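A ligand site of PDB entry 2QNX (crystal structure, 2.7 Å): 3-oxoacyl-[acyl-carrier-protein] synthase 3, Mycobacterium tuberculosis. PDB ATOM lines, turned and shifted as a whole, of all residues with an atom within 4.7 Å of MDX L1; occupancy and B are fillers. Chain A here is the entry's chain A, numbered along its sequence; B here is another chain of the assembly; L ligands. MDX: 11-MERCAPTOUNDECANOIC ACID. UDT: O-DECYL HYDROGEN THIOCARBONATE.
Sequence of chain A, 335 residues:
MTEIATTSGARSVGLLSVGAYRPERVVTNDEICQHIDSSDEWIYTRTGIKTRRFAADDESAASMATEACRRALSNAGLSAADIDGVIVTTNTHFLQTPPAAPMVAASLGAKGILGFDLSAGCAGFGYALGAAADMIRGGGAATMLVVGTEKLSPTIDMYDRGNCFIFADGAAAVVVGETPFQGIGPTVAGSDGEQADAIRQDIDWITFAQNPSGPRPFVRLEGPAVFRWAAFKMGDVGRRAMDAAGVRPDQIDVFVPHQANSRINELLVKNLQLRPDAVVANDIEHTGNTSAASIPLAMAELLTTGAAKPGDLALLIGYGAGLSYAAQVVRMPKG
N of Cys 122 lies close to S1 of MDX L1 (3.3 Å). SG of Cys 122 is covalently linked to S1 of MDX L1 (2.0 Å). The backbone NH of Phe 218 is in hydrogen-bond range of an oxygen (O1) of MDX L1 (3.2 Å). The backbone NH (N) of Ala 321 lies close to a sulfur (S1) of MDX L1 (3.6 Å).
A sulfur (S1) of MDX L1 lies close to a sulfur (S1) of UDT L2 (3.3 Å).
The side-chain sulfur (SG) of Cys 122 sits close to the side-chain hydroxyl (OG) of Ser 291, at 3.7 Å. NE1 of Trp 205 sits close to NE2 of Gln 201. The side-chain amide oxygen (OE1) of Gln 201 sits at hydrogen-bond distance from the backbone NH (N) of Gln 96 of chain B (3.0 Å). The side-chain hydroxyl (OG1) of Thr 155 lies within hydrogen-bond range of the backbone carbonyl oxygen (O) of Leu 152, at 2.9 Å. The backbone carbonyl oxygen of Thr 155 sits at hydrogen-bond distance from the backbone NH of Val 219. NE1 of Trp 205 is in hydrogen-bond range of OE1 of Gln 96 of chain B. The side-chain amide nitrogen (NE2) of Gln 96 of chain B lies within hydrogen-bond range of the backbone carbonyl oxygen (O) of Asn 91 (2.7 Å). The side-chain amide nitrogen of Asn 91 lies within hydrogen-bond range of the backbone carbonyl oxygen of Gly 121 (3.3 Å).
The backbone carbonyl oxygen of Pro 217 lies close to an oxygen (O1) of MDX L1. Residues that only touch MDX L1: Asn 91, Thr 92, Gly 121, Leu 152, Thr 155, Ile 199, Gln 201, Trp 205, Val 219, Ser 291, Gln 96 of chain B and Thr 97 of chain B. Within 4 Å of MDX L1: Asn 91, Thr 92, Gly 121, Cys 122, Leu 152, Thr 155, Ile 199, Gln 201, Trp 205, Pro 217, Phe 218, Val 219, Ser 291, Ala 321, Gln 96 of chain B and Thr 97 of chain B. Along chain A the residues within 4 Å of MDX L1 span positions 91 to 321.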
ATOM      1  N   ASN A  91     -20.026   9.514  29.907  1.00  0.00           N
ATOM      2  CA  ASN A  91     -20.526   9.980  28.621  1.00  0.00           C
ATOM      3  C   ASN A  91     -19.560   9.619  27.500  1.00  0.00           C
ATOM      4  O   ASN A  91     -19.836   9.878  26.322  1.00  0.00           O
ATOM      5  CB  ASN A  91     -20.741  11.491  28.617  1.00  0.00           C
ATOM      6  CG  ASN A  91     -21.698  11.953  29.701  1.00  0.00           C
ATOM      7  OD1 ASN A  91     -22.910  11.732  29.619  1.00  0.00           O
ATOM      8  ND2 ASN A  91     -21.159  12.612  30.723  1.00  0.00           N
ATOM      9  N   THR A  92     -18.422   9.040  27.846  1.00  0.00           N
ATOM     10  CA  THR A  92     -17.414   8.727  26.847  1.00  0.00           C
ATOM     11  C   THR A  92     -16.987   7.245  26.820  1.00  0.00           C
ATOM     12  O   THR A  92     -15.805   6.924  26.656  1.00  0.00           O
ATOM     13  CB  THR A  92     -16.191   9.691  26.903  1.00  0.00           C
ATOM     14  OG1 THR A  92     -15.674   9.754  28.230  1.00  0.00           O
ATOM     15  CG2 THR A  92     -16.584  11.077  26.454  1.00  0.00           C
ATOM     16  N   PHE A  94     -17.254   4.413  24.421  1.00  0.00           N
ATOM     17  CA  PHE A  94     -17.467   4.478  22.971  1.00  0.00           C
ATOM     18  C   PHE A  94     -17.898   3.167  22.333  1.00  0.00           C
ATOM     19  O   PHE A  94     -17.567   2.886  21.163  1.00  0.00           O
ATOM     20  CB  PHE A  94     -16.241   5.080  22.288  1.00  0.00           C
ATOM     21  CG  PHE A  94     -15.880   6.441  22.788  1.00  0.00           C
ATOM     22  CD1 PHE A  94     -14.635   6.685  23.338  1.00  0.00           C
ATOM     23  CD2 PHE A  94     -16.802   7.481  22.741  1.00  0.00           C
ATOM     24  CE1 PHE A  94     -14.302   7.953  23.819  1.00  0.00           C
ATOM     25  CE2 PHE A  94     -16.485   8.734  23.227  1.00  0.00           C
ATOM     26  CZ  PHE A  94     -15.233   8.971  23.754  1.00  0.00           C
ATOM     27  N   GLY A 121     -25.717  12.757  31.417  1.00  0.00           N
ATOM     28  CA  GLY A 121     -24.912  13.959  31.232  1.00  0.00           C
ATOM     29  C   GLY A 121     -24.040  14.175  32.453  1.00  0.00           C
ATOM     30  O   GLY A 121     -23.429  13.235  32.972  1.00  0.00           O
ATOM     31  N   CYS A 122     -24.015  15.417  32.939  1.00  0.00           N
ATOM     32  CA  CYS A 122     -23.246  15.708  34.125  1.00  0.00           C
ATOM     33  C   CYS A 122     -24.110  15.694  35.374  1.00  0.00           C
ATOM     34  O   CYS A 122     -23.760  16.291  36.390  1.00  0.00           O
ATOM     35  CB  CYS A 122     -22.496  17.027  33.963  1.00  0.00           C
ATOM     36  SG  CYS A 122     -21.350  16.941  32.584  1.00  0.00           S
ATOM     37  N   LEU A 152     -12.940  12.727  27.312  1.00  0.00           N
ATOM     38  CA  LEU A 152     -13.545  13.723  26.436  1.00  0.00           C
ATOM     39  C   LEU A 152     -12.615  14.213  25.331  1.00  0.00           C
ATOM     40  O   LEU A 152     -13.072  14.616  24.264  1.00  0.00           O
ATOM     41  CB  LEU A 152     -14.050  14.908  27.254  1.00  0.00           C
ATOM     42  CG  LEU A 152     -15.311  14.716  28.112  1.00  0.00           C
ATOM     43  CD1 LEU A 152     -15.294  15.624  29.329  1.00  0.00           C
ATOM     44  CD2 LEU A 152     -16.552  14.933  27.297  1.00  0.00           C
ATOM     45  N   THR A 155     -13.287  13.843  21.580  1.00  0.00           N
ATOM     46  CA  THR A 155     -14.554  14.388  21.095  1.00  0.00           C
ATOM     47  C   THR A 155     -14.513  15.901  20.882  1.00  0.00           C
ATOM     48  O   THR A 155     -15.505  16.510  20.472  1.00  0.00           O
ATOM     49  CB  THR A 155     -15.722  14.032  22.036  1.00  0.00           C
ATOM     50  OG1 THR A 155     -15.715  14.899  23.174  1.00  0.00           O
ATOM     51  CG2 THR A 155     -15.622  12.581  22.498  1.00  0.00           C
ATOM     52  N   PHE A 167     -13.389  20.863  27.957  1.00  0.00           N
ATOM     53  CA  PHE A 167     -13.417  19.470  28.350  1.00  0.00           C
ATOM     54  C   PHE A 167     -12.022  18.857  28.561  1.00  0.00           C
ATOM     55  O   PHE A 167     -11.031  19.322  28.001  1.00  0.00           O
ATOM     56  CB  PHE A 167     -14.292  18.668  27.367  1.00  0.00           C
ATOM     57  CG  PHE A 167     -15.717  19.189  27.282  1.00  0.00           C
ATOM     58  CD1 PHE A 167     -16.091  20.069  26.271  1.00  0.00           C
ATOM     59  CD2 PHE A 167     -16.662  18.831  28.231  1.00  0.00           C
ATOM     60  CE1 PHE A 167     -17.404  20.562  26.197  1.00  0.00           C
ATOM     61  CE2 PHE A 167     -17.978  19.312  28.169  1.00  0.00           C
ATOM     62  CZ  PHE A 167     -18.344  20.185  27.145  1.00  0.00           C
ATOM     63  N   ILE A 199     -26.430  20.909  24.860  1.00  0.00           N
ATOM     64  CA  ILE A 199     -25.199  20.125  24.946  1.00  0.00           C
ATOM     65  C   ILE A 199     -25.469  18.794  24.272  1.00  0.00           C
ATOM     66  O   ILE A 199     -26.359  18.045  24.697  1.00  0.00           O
ATOM     67  CB  ILE A 199     -24.777  19.864  26.393  1.00  0.00           C
ATOM     68  CG1 ILE A 199     -24.770  21.175  27.195  1.00  0.00           C
ATOM     69  CG2 ILE A 199     -23.404  19.171  26.435  1.00  0.00           C
ATOM     70  CD1 ILE A 199     -24.940  21.014  28.686  1.00  0.00           C
ATOM     71  N   ARG A 200     -24.683  18.494  23.243  1.00  0.00           N
ATOM     72  CA  ARG A 200     -24.976  17.370  22.362  1.00  0.00           C
ATOM     73  C   ARG A 200     -23.790  16.894  21.514  1.00  0.00           C
ATOM     74  O   ARG A 200     -22.774  17.582  21.367  1.00  0.00           O
ATOM     75  CB  ARG A 200     -26.121  17.741  21.420  1.00  0.00           C
ATOM     76  CG  ARG A 200     -25.681  18.632  20.278  1.00  0.00           C
ATOM     77  CD  ARG A 200     -26.828  19.373  19.649  1.00  0.00           C
ATOM     78  NE  ARG A 200     -26.505  19.725  18.265  1.00  0.00           N
ATOM     79  CZ  ARG A 200     -25.836  20.810  17.894  1.00  0.00           C
ATOM     80  NH1 ARG A 200     -25.391  21.688  18.780  1.00  0.00           N
ATOM     81  NH2 ARG A 200     -25.604  20.999  16.603  1.00  0.00           N
ATOM     82  N   GLN A 201     -23.963  15.703  20.954  1.00  0.00           N
ATOM     83  CA  GLN A 201     -23.133  15.200  19.876  1.00  0.00           C
ATOM     84  C   GLN A 201     -23.914  15.532  18.603  1.00  0.00           C
ATOM     85  O   GLN A 201     -25.040  15.081  18.430  1.00  0.00           O
ATOM     86  CB  GLN A 201     -22.958  13.687  20.038  1.00  0.00           C
ATOM     87  CG  GLN A 201     -22.362  12.967  18.847  1.00  0.00           C
ATOM     88  CD  GLN A 201     -22.049  11.512  19.134  1.00  0.00           C
ATOM     89  OE1 GLN A 201     -21.711  11.150  20.255  1.00  0.00           O
ATOM     90  NE2 GLN A 201     -22.150  10.669  18.116  1.00  0.00           N
ATOM     91  N   TRP A 205     -23.927   8.369  15.688  1.00  0.00           N
ATOM     92  CA  TRP A 205     -22.937   7.440  15.171  1.00  0.00           C
ATOM     93  C   TRP A 205     -23.425   6.652  13.950  1.00  0.00           C
ATOM     94  O   TRP A 205     -22.634   6.356  13.055  1.00  0.00           O
ATOM     95  CB  TRP A 205     -22.473   6.489  16.253  1.00  0.00           C
ATOM     96  CG  TRP A 205     -21.716   7.127  17.390  1.00  0.00           C
ATOM     97  CD1 TRP A 205     -22.106   7.180  18.687  1.00  0.00           C
ATOM     98  CD2 TRP A 205     -20.431   7.771  17.323  1.00  0.00           C
ATOM     99  NE1 TRP A 205     -21.150   7.834  19.444  1.00  0.00           N
ATOM    100  CE2 TRP A 205     -20.114   8.202  18.624  1.00  0.00           C
ATOM    101  CE3 TRP A 205     -19.522   8.029  16.283  1.00  0.00           C
ATOM    102  CZ2 TRP A 205     -18.929   8.885  18.929  1.00  0.00           C
ATOM    103  CZ3 TRP A 205     -18.334   8.702  16.587  1.00  0.00           C
ATOM    104  CH2 TRP A 205     -18.054   9.121  17.899  1.00  0.00           C
ATOM    105  N   ARG A 216     -17.230  14.256  10.647  1.00  0.00           N
ATOM    106  CA  ARG A 216     -17.329  13.371  11.795  1.00  0.00           C
ATOM    107  C   ARG A 216     -17.926  14.101  12.997  1.00  0.00           C
ATOM    108  O   ARG A 216     -17.813  15.322  13.094  1.00  0.00           O
ATOM    109  CB  ARG A 216     -15.953  12.807  12.145  1.00  0.00           C
ATOM    110  CG  ARG A 216     -14.937  13.813  12.624  1.00  0.00           C
ATOM    111  CD  ARG A 216     -14.023  13.212  13.669  1.00  0.00           C
ATOM    112  NE  ARG A 216     -14.586  13.301  15.016  1.00  0.00           N
ATOM    113  CZ  ARG A 216     -14.067  12.696  16.092  1.00  0.00           C
ATOM    114  NH1 ARG A 216     -12.994  11.936  15.973  1.00  0.00           N
ATOM    115  NH2 ARG A 216     -14.653  12.840  17.277  1.00  0.00           N
ATOM    116  N   PRO A 217     -18.569  13.358  13.923  1.00  0.00           N
ATOM    117  CA  PRO A 217     -19.248  13.981  15.057  1.00  0.00           C
ATOM    118  C   PRO A 217     -18.277  14.591  16.071  1.00  0.00           C
ATOM    119  O   PRO A 217     -17.149  14.117  16.208  1.00  0.00           O
ATOM    120  CB  PRO A 217     -20.009  12.828  15.706  1.00  0.00           C
ATOM    121  CG  PRO A 217     -19.981  11.720  14.701  1.00  0.00           C
ATOM    122  CD  PRO A 217     -18.709  11.887  13.965  1.00  0.00           C
ATOM    123  N   PHE A 218     -18.733  15.621  16.765  1.00  0.00           N
ATOM    124  CA  PHE A 218     -17.984  16.260  17.841  1.00  0.00           C
ATOM    125  C   PHE A 218     -18.944  16.678  18.938  1.00  0.00           C
ATOM    126  O   PHE A 218     -20.172  16.583  18.764  1.00  0.00           O
ATOM    127  CB  PHE A 218     -17.206  17.474  17.321  1.00  0.00           C
ATOM    128  CG  PHE A 218     -15.974  17.126  16.518  1.00  0.00           C
ATOM    129  CD1 PHE A 218     -14.855  16.587  17.139  1.00  0.00           C
ATOM    130  CD2 PHE A 218     -15.927  17.365  15.144  1.00  0.00           C
ATOM    131  CE1 PHE A 218     -13.727  16.275  16.397  1.00  0.00           C
ATOM    132  CE2 PHE A 218     -14.793  17.066  14.400  1.00  0.00           C
ATOM    133  CZ  PHE A 218     -13.693  16.521  15.026  1.00  0.00           C
ATOM    134  N   VAL A 219     -18.397  17.121  20.069  1.00  0.00           N
ATOM    135  CA  VAL A 219     -19.219  17.679  21.163  1.00  0.00           C
ATOM    136  C   VAL A 219     -19.522  19.149  20.852  1.00  0.00           C
ATOM    137  O   VAL A 219     -18.603  19.930  20.564  1.00  0.00           O
ATOM    138  CB  VAL A 219     -18.561  17.498  22.572  1.00  0.00           C
ATOM    139  CG1 VAL A 219     -17.195  18.191  22.647  1.00  0.00           C
ATOM    140  CG2 VAL A 219     -19.482  17.970  23.677  1.00  0.00           C
ATOM    141  N   SER A 291     -17.030  16.544  33.122  1.00  0.00           N
ATOM    142  CA  SER A 291     -18.375  16.006  33.036  1.00  0.00           C
ATOM    143  C   SER A 291     -18.768  15.117  34.228  1.00  0.00           C
ATOM    144  O   SER A 291     -18.562  15.511  35.375  1.00  0.00           O
ATOM    145  CB  SER A 291     -18.562  15.293  31.696  1.00  0.00           C
ATOM    146  OG  SER A 291     -18.249  16.189  30.652  1.00  0.00           O
ATOM    147  N   GLY A 320     -26.149  19.652  33.447  1.00  0.00           N
ATOM    148  CA  GLY A 320     -25.551  19.583  32.132  1.00  0.00           C
ATOM    149  C   GLY A 320     -26.388  18.925  31.071  1.00  0.00           C
ATOM    150  O   GLY A 320     -27.568  19.234  30.933  1.00  0.00           O
ATOM    151  N   ALA A 321     -25.768  18.015  30.326  1.00  0.00           N
ATOM    152  CA  ALA A 321     -26.355  17.427  29.118  1.00  0.00           C
ATOM    153  C   ALA A 321     -27.799  16.916  29.247  1.00  0.00           C
ATOM    154  O   ALA A 321     -28.247  16.502  30.325  1.00  0.00           O
ATOM    155  CB  ALA A 321     -25.455  16.344  28.558  1.00  0.00           C
ATOM    156  N   GLN B  96     -23.527   9.747  22.236  1.00  0.00           N
ATOM    157  CA  GLN B  96     -22.797   9.778  23.503  1.00  0.00           C
ATOM    158  C   GLN B  96     -23.498  10.697  24.500  1.00  0.00           C
ATOM    159  O   GLN B  96     -23.644  10.353  25.676  1.00  0.00           O
ATOM    160  CB  GLN B  96     -21.341  10.201  23.310  1.00  0.00           C
ATOM    161  CG  GLN B  96     -20.493   9.200  22.524  1.00  0.00           C
ATOM    162  CD  GLN B  96     -20.321   7.854  23.202  1.00  0.00           C
ATOM    163  OE1 GLN B  96     -20.449   6.810  22.562  1.00  0.00           O
ATOM    164  NE2 GLN B  96     -20.020   7.870  24.489  1.00  0.00           N
ATOM    165  N   THR B  97     -23.933  11.861  24.018  1.00  0.00           N
ATOM    166  CA  THR B  97     -24.806  12.773  24.762  1.00  0.00           C
ATOM    167  C   THR B  97     -25.606  13.619  23.759  1.00  0.00           C
ATOM    168  O   THR B  97     -25.147  13.830  22.632  1.00  0.00           O
ATOM    169  CB  THR B  97     -24.003  13.654  25.785  1.00  0.00           C
ATOM    170  OG1 THR B  97     -24.639  13.617  27.073  1.00  0.00           O
ATOM    171  CG2 THR B  97     -23.858  15.112  25.304  1.00  0.00           C
ATOM    172  N   ILE B 206     -14.795   5.986  18.273  1.00  0.00           N
ATOM    173  CA  ILE B 206     -13.733   6.960  18.021  1.00  0.00           C
ATOM    174  C   ILE B 206     -12.658   6.389  17.094  1.00  0.00           C
ATOM    175  O   ILE B 206     -12.205   7.081  16.172  1.00  0.00           O
ATOM    176  CB  ILE B 206     -13.097   7.516  19.321  1.00  0.00           C
ATOM    177  CG1 ILE B 206     -14.146   8.302  20.141  1.00  0.00           C
ATOM    178  CG2 ILE B 206     -11.873   8.387  19.015  1.00  0.00           C
ATOM    179  CD1 ILE B 206     -14.632   9.597  19.492  1.00  0.00           C
HETATM  180  O1  MDX L   1     -19.178  13.162  18.841  1.00  0.00           O
HETATM  181  C11 MDX L   1     -18.724  12.963  19.986  1.00  0.00           C
HETATM  182  O2  MDX L   1     -17.969  12.028  20.328  1.00  0.00           O
HETATM  183  C10 MDX L   1     -19.126  13.953  21.071  1.00  0.00           C
HETATM  184  C9  MDX L   1     -20.065  13.309  22.079  1.00  0.00           C
HETATM  185  C8  MDX L   1     -20.229  14.200  23.297  1.00  0.00           C
HETATM  186  C7  MDX L   1     -19.021  14.040  24.214  1.00  0.00           C
HETATM  187  C6  MDX L   1     -19.437  13.388  25.530  1.00  0.00           C
HETATM  188  C5  MDX L   1     -20.434  14.258  26.290  1.00  0.00           C
HETATM  189  C4  MDX L   1     -19.767  15.517  26.810  1.00  0.00           C
HETATM  190  C3  MDX L   1     -20.809  16.606  27.046  1.00  0.00           C
HETATM  191  C2  MDX L   1     -21.618  16.305  28.298  1.00  0.00           C
HETATM  192  C1  MDX L   1     -21.089  17.109  29.454  1.00  0.00           C
HETATM  193  S1  MDX L   1     -22.274  17.173  30.824  1.00  0.00           S
HETATM  194  C11 UDT L   2     -17.247  31.799  26.272  1.00  0.00           C
HETATM  195  C10 UDT L   2     -18.013  31.385  27.535  1.00  0.00           C
HETATM  196  C9  UDT L   2     -17.626  29.956  27.956  1.00  0.00           C
HETATM  197  C8  UDT L   2     -18.804  28.990  27.825  1.00  0.00           C
HETATM  198  C7  UDT L   2     -19.612  28.918  29.121  1.00  0.00           C
HETATM  199  C6  UDT L   2     -20.600  27.745  29.097  1.00  0.00           C
HETATM  200  C5  UDT L   2     -20.131  26.616  30.027  1.00  0.00           C
HETATM  201  C4  UDT L   2     -21.106  25.436  30.000  1.00  0.00           C
HETATM  202  C3  UDT L   2     -20.343  24.111  29.882  1.00  0.00           C
HETATM  203  C2  UDT L   2     -21.144  22.949  30.460  1.00  0.00           C
HETATM  204  O2  UDT L   2     -20.805  21.699  29.817  1.00  0.00           O
HETATM  205  C1  UDT L   2     -20.980  20.630  30.649  1.00  0.00           C
HETATM  206  O1  UDT L   2     -20.083  19.815  30.832  1.00  0.00           O
HETATM  207  S1  UDT L   2     -22.489  20.423  31.465  1.00  0.00           S
